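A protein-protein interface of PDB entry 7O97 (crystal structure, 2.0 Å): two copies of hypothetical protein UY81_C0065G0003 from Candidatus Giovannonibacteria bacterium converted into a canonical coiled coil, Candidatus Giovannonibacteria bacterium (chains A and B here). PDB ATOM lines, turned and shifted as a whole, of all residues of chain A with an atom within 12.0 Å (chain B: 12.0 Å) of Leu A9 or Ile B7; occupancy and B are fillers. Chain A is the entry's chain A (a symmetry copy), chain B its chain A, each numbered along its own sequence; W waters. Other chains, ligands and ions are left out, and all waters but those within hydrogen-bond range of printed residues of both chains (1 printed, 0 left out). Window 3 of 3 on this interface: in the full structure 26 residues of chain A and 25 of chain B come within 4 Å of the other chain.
Among the printed residues, merely in contact across the chains: Leu A9 with Ile B7, Leu A9 with Leu B9, Leu A9 with Leu B12, Val A13 with Leu B12, Val A16 with Val B16 and Phe A20 with Val B16.
Of chain B, only Ile B7 (3.7 Å), Leu B9 (3.8 Å) and Leu B12 (3.8 Å) come within 4 Å of Leu A9. Ile B7 touches one residue of chain A. No residue of chain B comes within 4 Å of Ile A7. Thr A8 touches none of the printed residues of chain B. No residue of chain B comes within 4 Å of Glu A10. No residue of chain B comes within 4 Å of Lys A11. No residue of chain B comes within 4 Å of Leu A12. Of chain B, only Leu B12 comes within 4 Å of Val A13. No residue of chain A comes within 4 Å of Lys B5. No residue of chain A comes within 4 Å of Pro B6. No residue of chain A comes within 4 Å of Lys B11. Of chain A, only Leu A9 (3.8 Å) and Val A13 (3.8 Å) come within 4 Å of Leu B12. Of the printed residues of chain A, Val B16 touches Val A16 (3.97 Å) and Phe A20 (3.7 Å). Of the printed residues of chain B, Phe A20 touches Val B16 (3.7 Å). Of the printed residues of chain B, Val A16 touches Val B16. The nearest residue of chain A that does not touch Ile B7 is Glu A10 (4.3 Å). The nearest printed residue of chain A that does not touch Val B16 is Leu A12 (6.3 Å).
Of the 15 printed residues of chain A, 4 touch a printed residue of chain B. Hydrophobic or aromatic side chains of chain A within 4 Å of the printed part of chain B: Leu A9, Val A13, Val A16 and Phe A20. Among the printed residues, 6 pairs touch across the chains. Among the printed residues, no Asp or Glu carboxylate lies within 4 Å of a Lys or Arg side-chain nitrogen of the other chain.
Leu A9 touches Ile B7, but with the chains exchanged Ile A7 does not touch Leu B9 (9.3 Å). Leu A9 touches Leu B12, but with the chains exchanged Leu A12 does not touch Leu B9 (5.9 Å). Val A13 touches Leu B12, but with the chains exchanged Leu A12 does not touch Val B13 (7.5 Å). Val A16 touches its own counterpart, Val B16.
Water W1 lies within hydrogen-bond range of OE2 of Glu A10 (3.3 Å) and O of Ile B7 (3.4 Å).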
ATOM      1  N   LYS A   5     -31.700 -23.603 -17.282  1.00  0.00           N
ATOM      2  CA  LYS A   5     -30.627 -22.683 -17.757  1.00  0.00           C
ATOM      3  C   LYS A   5     -30.678 -22.380 -19.307  1.00  0.00           C
ATOM      4  O   LYS A   5     -29.785 -22.777 -20.085  1.00  0.00           O
ATOM      5  CB  LYS A   5     -29.252 -23.241 -17.307  1.00  0.00           C
ATOM      6  CG  LYS A   5     -28.072 -22.501 -17.916  1.00  0.00           C
ATOM      7  CD  LYS A   5     -26.899 -22.316 -16.980  1.00  0.00           C
ATOM      8  CE  LYS A   5     -26.038 -21.179 -17.530  1.00  0.00           C
ATOM      9  NZ  LYS A   5     -24.669 -21.067 -16.955  1.00  0.00           N
ATOM     10  N   PRO A   6     -31.716 -21.644 -19.758  1.00  0.00           N
ATOM     11  CA  PRO A   6     -31.815 -21.329 -21.201  1.00  0.00           C
ATOM     12  C   PRO A   6     -30.823 -20.162 -21.538  1.00  0.00           C
ATOM     13  O   PRO A   6     -31.224 -19.040 -21.824  1.00  0.00           O
ATOM     14  CB  PRO A   6     -33.319 -20.982 -21.383  1.00  0.00           C
ATOM     15  CG  PRO A   6     -33.963 -21.244 -20.040  1.00  0.00           C
ATOM     16  CD  PRO A   6     -32.884 -21.143 -19.013  1.00  0.00           C
ATOM     17  N   ILE A   7     -29.522 -20.443 -21.435  1.00  0.00           N
ATOM     18  CA  ILE A   7     -28.466 -19.406 -21.549  1.00  0.00           C
ATOM     19  C   ILE A   7     -28.492 -18.704 -22.910  1.00  0.00           C
ATOM     20  O   ILE A   7     -28.323 -19.339 -23.944  1.00  0.00           O
ATOM     21  CB  ILE A   7     -27.054 -19.960 -21.213  1.00  0.00           C
ATOM     22  CG1 ILE A   7     -25.979 -18.896 -21.415  1.00  0.00           C
ATOM     23  CG2 ILE A   7     -26.713 -21.196 -22.030  1.00  0.00           C
ATOM     24  CD1 ILE A   7     -24.773 -19.145 -20.543  1.00  0.00           C
ATOM     25  N   THR A   8     -28.742 -17.399 -22.872  1.00  0.00           N
ATOM     26  CA  THR A   8     -29.084 -16.616 -24.057  1.00  0.00           C
ATOM     27  C   THR A   8     -27.833 -15.901 -24.592  1.00  0.00           C
ATOM     28  O   THR A   8     -26.843 -15.711 -23.866  1.00  0.00           O
ATOM     29  CB  THR A   8     -30.107 -15.484 -23.794  1.00  0.00           C
ATOM     30  OG1 THR A   8     -29.565 -14.656 -22.778  1.00  0.00           O
ATOM     31  CG2 THR A   8     -31.519 -15.981 -23.404  1.00  0.00           C
ATOM     32  N   LEU A   9     -27.962 -15.461 -25.838  1.00  0.00           N
ATOM     33  CA  LEU A   9     -27.090 -14.446 -26.524  1.00  0.00           C
ATOM     34  C   LEU A   9     -26.759 -13.189 -25.713  1.00  0.00           C
ATOM     35  O   LEU A   9     -25.611 -12.993 -25.456  1.00  0.00           O
ATOM     36  CB  LEU A   9     -27.714 -13.987 -27.810  1.00  0.00           C
ATOM     37  CG  LEU A   9     -26.768 -13.056 -28.633  1.00  0.00           C
ATOM     38  CD1 LEU A   9     -25.407 -13.657 -29.004  1.00  0.00           C
ATOM     39  CD2 LEU A   9     -27.508 -12.599 -29.871  1.00  0.00           C
ATOM     40  N   GLU A  10     -27.713 -12.355 -25.242  1.00  0.00           N
ATOM     41  CA  GLU A  10     -27.260 -11.144 -24.485  1.00  0.00           C
ATOM     42  C   GLU A  10     -26.554 -11.510 -23.221  1.00  0.00           C
ATOM     43  O   GLU A  10     -25.579 -10.850 -22.828  1.00  0.00           O
ATOM     44  CB  GLU A  10     -28.320 -10.025 -24.271  1.00  0.00           C
ATOM     45  CG  GLU A  10     -27.866  -8.877 -23.290  1.00  0.00           C
ATOM     46  CD  GLU A  10     -26.570  -8.058 -23.640  1.00  0.00           C
ATOM     47  OE1 GLU A  10     -25.574  -7.995 -22.769  1.00  0.00           O
ATOM     48  OE2 GLU A  10     -26.496  -7.447 -24.801  1.00  0.00           O
ATOM     49  N   LYS A  11     -26.910 -12.637 -22.626  1.00  0.00           N
ATOM     50  CA  LYS A  11     -26.162 -13.094 -21.477  1.00  0.00           C
ATOM     51  C   LYS A  11     -24.675 -13.459 -21.760  1.00  0.00           C
ATOM     52  O   LYS A  11     -23.702 -13.069 -21.050  1.00  0.00           O
ATOM     53  CB  LYS A  11     -26.920 -14.278 -20.809  1.00  0.00           C
ATOM     54  CG  LYS A  11     -26.762 -14.362 -19.288  1.00  0.00           C
ATOM     55  CD  LYS A  11     -25.695 -13.434 -18.660  1.00  0.00           C
ATOM     56  N   LEU A  12     -24.441 -14.207 -22.833  1.00  0.00           N
ATOM     57  CA  LEU A  12     -23.097 -14.547 -23.188  1.00  0.00           C
ATOM     58  C   LEU A  12     -22.363 -13.311 -23.617  1.00  0.00           C
ATOM     59  O   LEU A  12     -21.218 -13.106 -23.238  1.00  0.00           O
ATOM     60  CB  LEU A  12     -23.197 -15.641 -24.286  1.00  0.00           C
ATOM     61  CG  LEU A  12     -21.879 -16.220 -24.759  1.00  0.00           C
ATOM     62  CD1 LEU A  12     -21.193 -17.021 -23.657  1.00  0.00           C
ATOM     63  CD2 LEU A  12     -22.182 -17.087 -26.043  1.00  0.00           C
ATOM     64  N   VAL A  13     -23.018 -12.426 -24.343  1.00  0.00           N
ATOM     65  CA  VAL A  13     -22.434 -11.061 -24.537  1.00  0.00           C
ATOM     66  C   VAL A  13     -21.864 -10.503 -23.309  1.00  0.00           C
ATOM     67  O   VAL A  13     -20.695 -10.108 -23.237  1.00  0.00           O
ATOM     68  CB  VAL A  13     -23.406 -10.013 -25.240  1.00  0.00           C
ATOM     69  CG1 VAL A  13     -22.797  -8.601 -25.303  1.00  0.00           C
ATOM     70  CG2 VAL A  13     -23.999 -10.417 -26.569  1.00  0.00           C
ATOM     71  N   SER A  14     -22.636 -10.527 -22.169  1.00  0.00           N
ATOM     72  CA  SER A  14     -22.113  -9.954 -20.943  1.00  0.00           C
ATOM     73  C   SER A  14     -21.066 -10.758 -20.373  1.00  0.00           C
ATOM     74  O   SER A  14     -20.028 -10.251 -19.932  1.00  0.00           O
ATOM     75  CB  SER A  14     -23.152  -9.809 -19.774  1.00  0.00           C
ATOM     76  OG  SER A  14     -24.412  -9.739 -20.283  1.00  0.00           O
ATOM     77  N   MET A  15     -21.249 -12.092 -20.430  1.00  0.00           N
ATOM     78  CA  MET A  15     -20.171 -12.979 -19.933  1.00  0.00           C
ATOM     79  C   MET A  15     -18.866 -12.833 -20.647  1.00  0.00           C
ATOM     80  O   MET A  15     -17.772 -12.815 -20.025  1.00  0.00           O
ATOM     81  CB  MET A  15     -20.594 -14.468 -19.962  1.00  0.00           C
ATOM     82  CG  MET A  15     -21.927 -14.753 -19.237  1.00  0.00           C
ATOM     83  SD  MET A  15     -22.609 -16.391 -19.664  1.00  0.00           S
ATOM     84  CE  MET A  15     -21.317 -17.280 -18.885  1.00  0.00           C
ATOM     85  N   VAL A  16     -18.964 -12.669 -21.971  1.00  0.00           N
ATOM     86  CA  VAL A  16     -17.739 -12.387 -22.745  1.00  0.00           C
ATOM     87  C   VAL A  16     -17.075 -11.078 -22.302  1.00  0.00           C
ATOM     88  O   VAL A  16     -15.872 -11.012 -21.894  1.00  0.00           O
ATOM     89  CB  VAL A  16     -18.044 -12.461 -24.259  1.00  0.00           C
ATOM     90  CG1 VAL A  16     -16.890 -11.974 -25.134  1.00  0.00           C
ATOM     91  CG2 VAL A  16     -18.548 -13.788 -24.698  1.00  0.00           C
ATOM     92  N   ALA A  17     -17.876  -9.988 -22.296  1.00  0.00           N
ATOM     93  CA  ALA A  17     -17.302  -8.742 -21.784  1.00  0.00           C
ATOM     94  C   ALA A  17     -16.533  -8.823 -20.469  1.00  0.00           C
ATOM     95  O   ALA A  17     -15.356  -8.474 -20.396  1.00  0.00           O
ATOM     96  CB  ALA A  17     -18.322  -7.632 -21.748  1.00  0.00           C
ATOM     97  N   VAL A  18     -17.199  -9.297 -19.394  1.00  0.00           N
ATOM     98  CA  VAL A  18     -16.640  -9.345 -18.105  1.00  0.00           C
ATOM     99  C   VAL A  18     -15.493 -10.354 -18.095  1.00  0.00           C
ATOM    100  O   VAL A  18     -14.433 -10.099 -17.569  1.00  0.00           O
ATOM    101  CB  VAL A  18     -17.751  -9.731 -17.059  1.00  0.00           C
ATOM    102  CG1 VAL A  18     -17.146  -9.813 -15.647  1.00  0.00           C
ATOM    103  CG2 VAL A  18     -18.839  -8.696 -17.123  1.00  0.00           C
ATOM    104  N   PHE A  20     -13.344 -11.205 -20.501  1.00  0.00           N
ATOM    105  CA  PHE A  20     -12.220 -10.533 -21.048  1.00  0.00           C
ATOM    106  C   PHE A  20     -11.665  -9.460 -20.175  1.00  0.00           C
ATOM    107  O   PHE A  20     -10.451  -9.364 -19.991  1.00  0.00           O
ATOM    108  CB  PHE A  20     -12.459  -9.879 -22.447  1.00  0.00           C
ATOM    109  CG  PHE A  20     -12.363 -10.884 -23.632  1.00  0.00           C
ATOM    110  CD1 PHE A  20     -11.348 -11.797 -23.695  1.00  0.00           C
ATOM    111  CD2 PHE A  20     -13.309 -10.907 -24.632  1.00  0.00           C
ATOM    112  CE1 PHE A  20     -11.258 -12.742 -24.755  1.00  0.00           C
ATOM    113  CE2 PHE A  20     -13.246 -11.864 -25.642  1.00  0.00           C
ATOM    114  CZ  PHE A  20     -12.209 -12.774 -25.695  1.00  0.00           C
ATOM    115  N   LYS B   5     -28.023  -0.713 -31.573  1.00  0.00           N
ATOM    116  CA  LYS B   5     -26.995  -1.781 -31.418  1.00  0.00           C
ATOM    117  C   LYS B   5     -27.593  -3.237 -31.281  1.00  0.00           C
ATOM    118  O   LYS B   5     -27.496  -3.891 -30.222  1.00  0.00           O
ATOM    119  CB  LYS B   5     -26.059  -1.410 -30.238  1.00  0.00           C
ATOM    120  CG  LYS B   5     -25.104  -2.528 -29.852  1.00  0.00           C
ATOM    121  CD  LYS B   5     -23.721  -2.060 -29.458  1.00  0.00           C
ATOM    122  CE  LYS B   5     -22.773  -3.253 -29.579  1.00  0.00           C
ATOM    123  NZ  LYS B   5     -21.449  -3.098 -28.915  1.00  0.00           N
ATOM    124  N   PRO B   6     -28.193  -3.764 -32.370  1.00  0.00           N
ATOM    125  CA  PRO B   6     -28.771  -5.124 -32.298  1.00  0.00           C
ATOM    126  C   PRO B   6     -27.614  -6.176 -32.409  1.00  0.00           C
ATOM    127  O   PRO B   6     -27.477  -6.879 -33.404  1.00  0.00           O
ATOM    128  CB  PRO B   6     -29.783  -5.138 -33.478  1.00  0.00           C
ATOM    129  CG  PRO B   6     -29.769  -3.736 -34.044  1.00  0.00           C
ATOM    130  CD  PRO B   6     -28.455  -3.131 -33.674  1.00  0.00           C
ATOM    131  N   ILE B   7     -26.754  -6.221 -31.389  1.00  0.00           N
ATOM    132  CA  ILE B   7     -25.513  -7.033 -31.421  1.00  0.00           C
ATOM    133  C   ILE B   7     -25.806  -8.526 -31.601  1.00  0.00           C
ATOM    134  O   ILE B   7     -26.477  -9.135 -30.776  1.00  0.00           O
ATOM    135  CB  ILE B   7     -24.602  -6.770 -30.190  1.00  0.00           C
ATOM    136  CG1 ILE B   7     -23.374  -7.675 -30.207  1.00  0.00           C
ATOM    137  CG2 ILE B   7     -25.347  -6.940 -28.876  1.00  0.00           C
ATOM    138  CD1 ILE B   7     -22.213  -7.060 -29.465  1.00  0.00           C
ATOM    139  N   THR B   8     -25.319  -9.072 -32.710  1.00  0.00           N
ATOM    140  CA  THR B   8     -25.721 -10.389 -33.197  1.00  0.00           C
ATOM    141  C   THR B   8     -24.693 -11.446 -32.765  1.00  0.00           C
ATOM    142  O   THR B   8     -23.537 -11.122 -32.442  1.00  0.00           O
ATOM    143  CB  THR B   8     -25.783 -10.501 -34.740  1.00  0.00           C
ATOM    144  OG1 THR B   8     -24.504 -10.145 -35.239  1.00  0.00           O
ATOM    145  CG2 THR B   8     -26.888  -9.640 -35.397  1.00  0.00           C
ATOM    146  N   LEU B   9     -25.140 -12.693 -32.854  1.00  0.00           N
ATOM    147  CA  LEU B   9     -24.308 -13.945 -32.845  1.00  0.00           C
ATOM    148  C   LEU B   9     -23.062 -13.928 -33.736  1.00  0.00           C
ATOM    149  O   LEU B   9     -22.004 -14.039 -33.198  1.00  0.00           O
ATOM    150  CB  LEU B   9     -25.127 -15.134 -33.257  1.00  0.00           C
ATOM    151  CG  LEU B   9     -24.346 -16.478 -33.106  1.00  0.00           C
ATOM    152  CD1 LEU B   9     -23.820 -16.783 -31.698  1.00  0.00           C
ATOM    153  CD2 LEU B   9     -25.228 -17.601 -33.604  1.00  0.00           C
ATOM    154  N   GLU B  10     -23.126 -13.733 -35.072  1.00  0.00           N
ATOM    155  CA  GLU B  10     -21.839 -13.766 -35.838  1.00  0.00           C
ATOM    156  C   GLU B  10     -20.924 -12.658 -35.435  1.00  0.00           C
ATOM    157  O   GLU B  10     -19.698 -12.841 -35.376  1.00  0.00           O
ATOM    158  CB  GLU B  10     -21.957 -13.906 -37.383  1.00  0.00           C
ATOM    159  CG  GLU B  10     -20.598 -13.716 -38.160  1.00  0.00           C
ATOM    160  CD  GLU B  10     -19.398 -14.675 -37.821  1.00  0.00           C
ATOM    161  OE1 GLU B  10     -18.236 -14.168 -37.438  1.00  0.00           O
ATOM    162  OE2 GLU B  10     -19.572 -15.975 -37.920  1.00  0.00           O
ATOM    163  N   LYS B  11     -21.476 -11.534 -35.005  1.00  0.00           N
ATOM    164  CA  LYS B  11     -20.628 -10.488 -34.479  1.00  0.00           C
ATOM    165  C   LYS B  11     -19.851 -10.858 -33.182  1.00  0.00           C
ATOM    166  O   LYS B  11     -18.616 -10.642 -33.009  1.00  0.00           O
ATOM    167  CB  LYS B  11     -21.470  -9.193 -34.288  1.00  0.00           C
ATOM    168  CG  LYS B  11     -20.696  -7.889 -34.505  1.00  0.00           C
ATOM    169  CD  LYS B  11     -19.160  -8.021 -34.638  1.00  0.00           C
ATOM    170  N   LEU B  12     -20.549 -11.459 -32.223  1.00  0.00           N
ATOM    171  CA  LEU B  12     -19.897 -11.873 -31.018  1.00  0.00           C
ATOM    172  C   LEU B  12     -18.937 -12.986 -31.322  1.00  0.00           C
ATOM    173  O   LEU B  12     -17.821 -12.997 -30.822  1.00  0.00           O
ATOM    174  CB  LEU B  12     -21.024 -12.261 -30.021  1.00  0.00           C
ATOM    175  CG  LEU B  12     -20.566 -12.655 -28.632  1.00  0.00           C
ATOM    176  CD1 LEU B  12     -19.957 -11.470 -27.887  1.00  0.00           C
ATOM    177  CD2 LEU B  12     -21.813 -13.268 -27.883  1.00  0.00           C
ATOM    178  N   VAL B  13     -19.307 -13.896 -32.201  1.00  0.00           N
ATOM    179  CA  VAL B  13     -18.284 -14.840 -32.755  1.00  0.00           C
ATOM    180  C   VAL B  13     -17.022 -14.179 -33.093  1.00  0.00           C
ATOM    181  O   VAL B  13     -15.935 -14.548 -32.637  1.00  0.00           O
ATOM    182  CB  VAL B  13     -18.795 -15.745 -33.962  1.00  0.00           C
ATOM    183  CG1 VAL B  13     -17.670 -16.604 -34.566  1.00  0.00           C
ATOM    184  CG2 VAL B  13     -20.043 -16.560 -33.723  1.00  0.00           C
ATOM    185  N   SER B  14     -17.076 -13.038 -33.863  1.00  0.00           N
ATOM    186  CA  SER B  14     -15.842 -12.377 -34.243  1.00  0.00           C
ATOM    187  C   SER B  14     -15.214 -11.718 -33.129  1.00  0.00           C
ATOM    188  O   SER B  14     -13.996 -11.801 -32.930  1.00  0.00           O
ATOM    189  CB  SER B  14     -15.992 -11.240 -35.314  1.00  0.00           C
ATOM    190  OG  SER B  14     -17.114 -11.448 -36.055  1.00  0.00           O
ATOM    191  N   MET B  15     -16.044 -11.087 -32.275  1.00  0.00           N
ATOM    192  CA  MET B  15     -15.470 -10.457 -31.063  1.00  0.00           C
ATOM    193  C   MET B  15     -14.768 -11.402 -30.142  1.00  0.00           C
ATOM    194  O   MET B  15     -13.671 -11.106 -29.601  1.00  0.00           O
ATOM    195  CB  MET B  15     -16.539  -9.677 -30.260  1.00  0.00           C
ATOM    196  CG  MET B  15     -17.325  -8.649 -31.101  1.00  0.00           C
ATOM    197  SD  MET B  15     -18.842  -8.083 -30.260  1.00  0.00           S
ATOM    198  CE  MET B  15     -17.983  -7.255 -28.978  1.00  0.00           C
ATOM    199  N   VAL B  16     -15.367 -12.589 -29.991  1.00  0.00           N
ATOM    200  CA  VAL B  16     -14.684 -13.636 -29.205  1.00  0.00           C
ATOM    201  C   VAL B  16     -13.337 -14.026 -29.826  1.00  0.00           C
ATOM    202  O   VAL B  16     -12.235 -13.957 -29.195  1.00  0.00           O
ATOM    203  CB  VAL B  16     -15.641 -14.827 -28.970  1.00  0.00           C
ATOM    204  CG1 VAL B  16     -14.954 -16.043 -28.352  1.00  0.00           C
ATOM    205  CG2 VAL B  16     -16.878 -14.458 -28.234  1.00  0.00           C
ATOM    206  N   ALA B  17     -13.376 -14.382 -31.130  1.00  0.00           N
ATOM    207  CA  ALA B  17     -12.095 -14.665 -31.782  1.00  0.00           C
ATOM    208  C   ALA B  17     -10.967 -13.662 -31.554  1.00  0.00           C
ATOM    209  O   ALA B  17      -9.896 -14.011 -31.059  1.00  0.00           O
ATOM    210  CB  ALA B  17     -12.269 -14.961 -33.250  1.00  0.00           C
HETATM  211  O   HOH W   1     -27.563  -8.941 -27.589  1.00  0.00           O
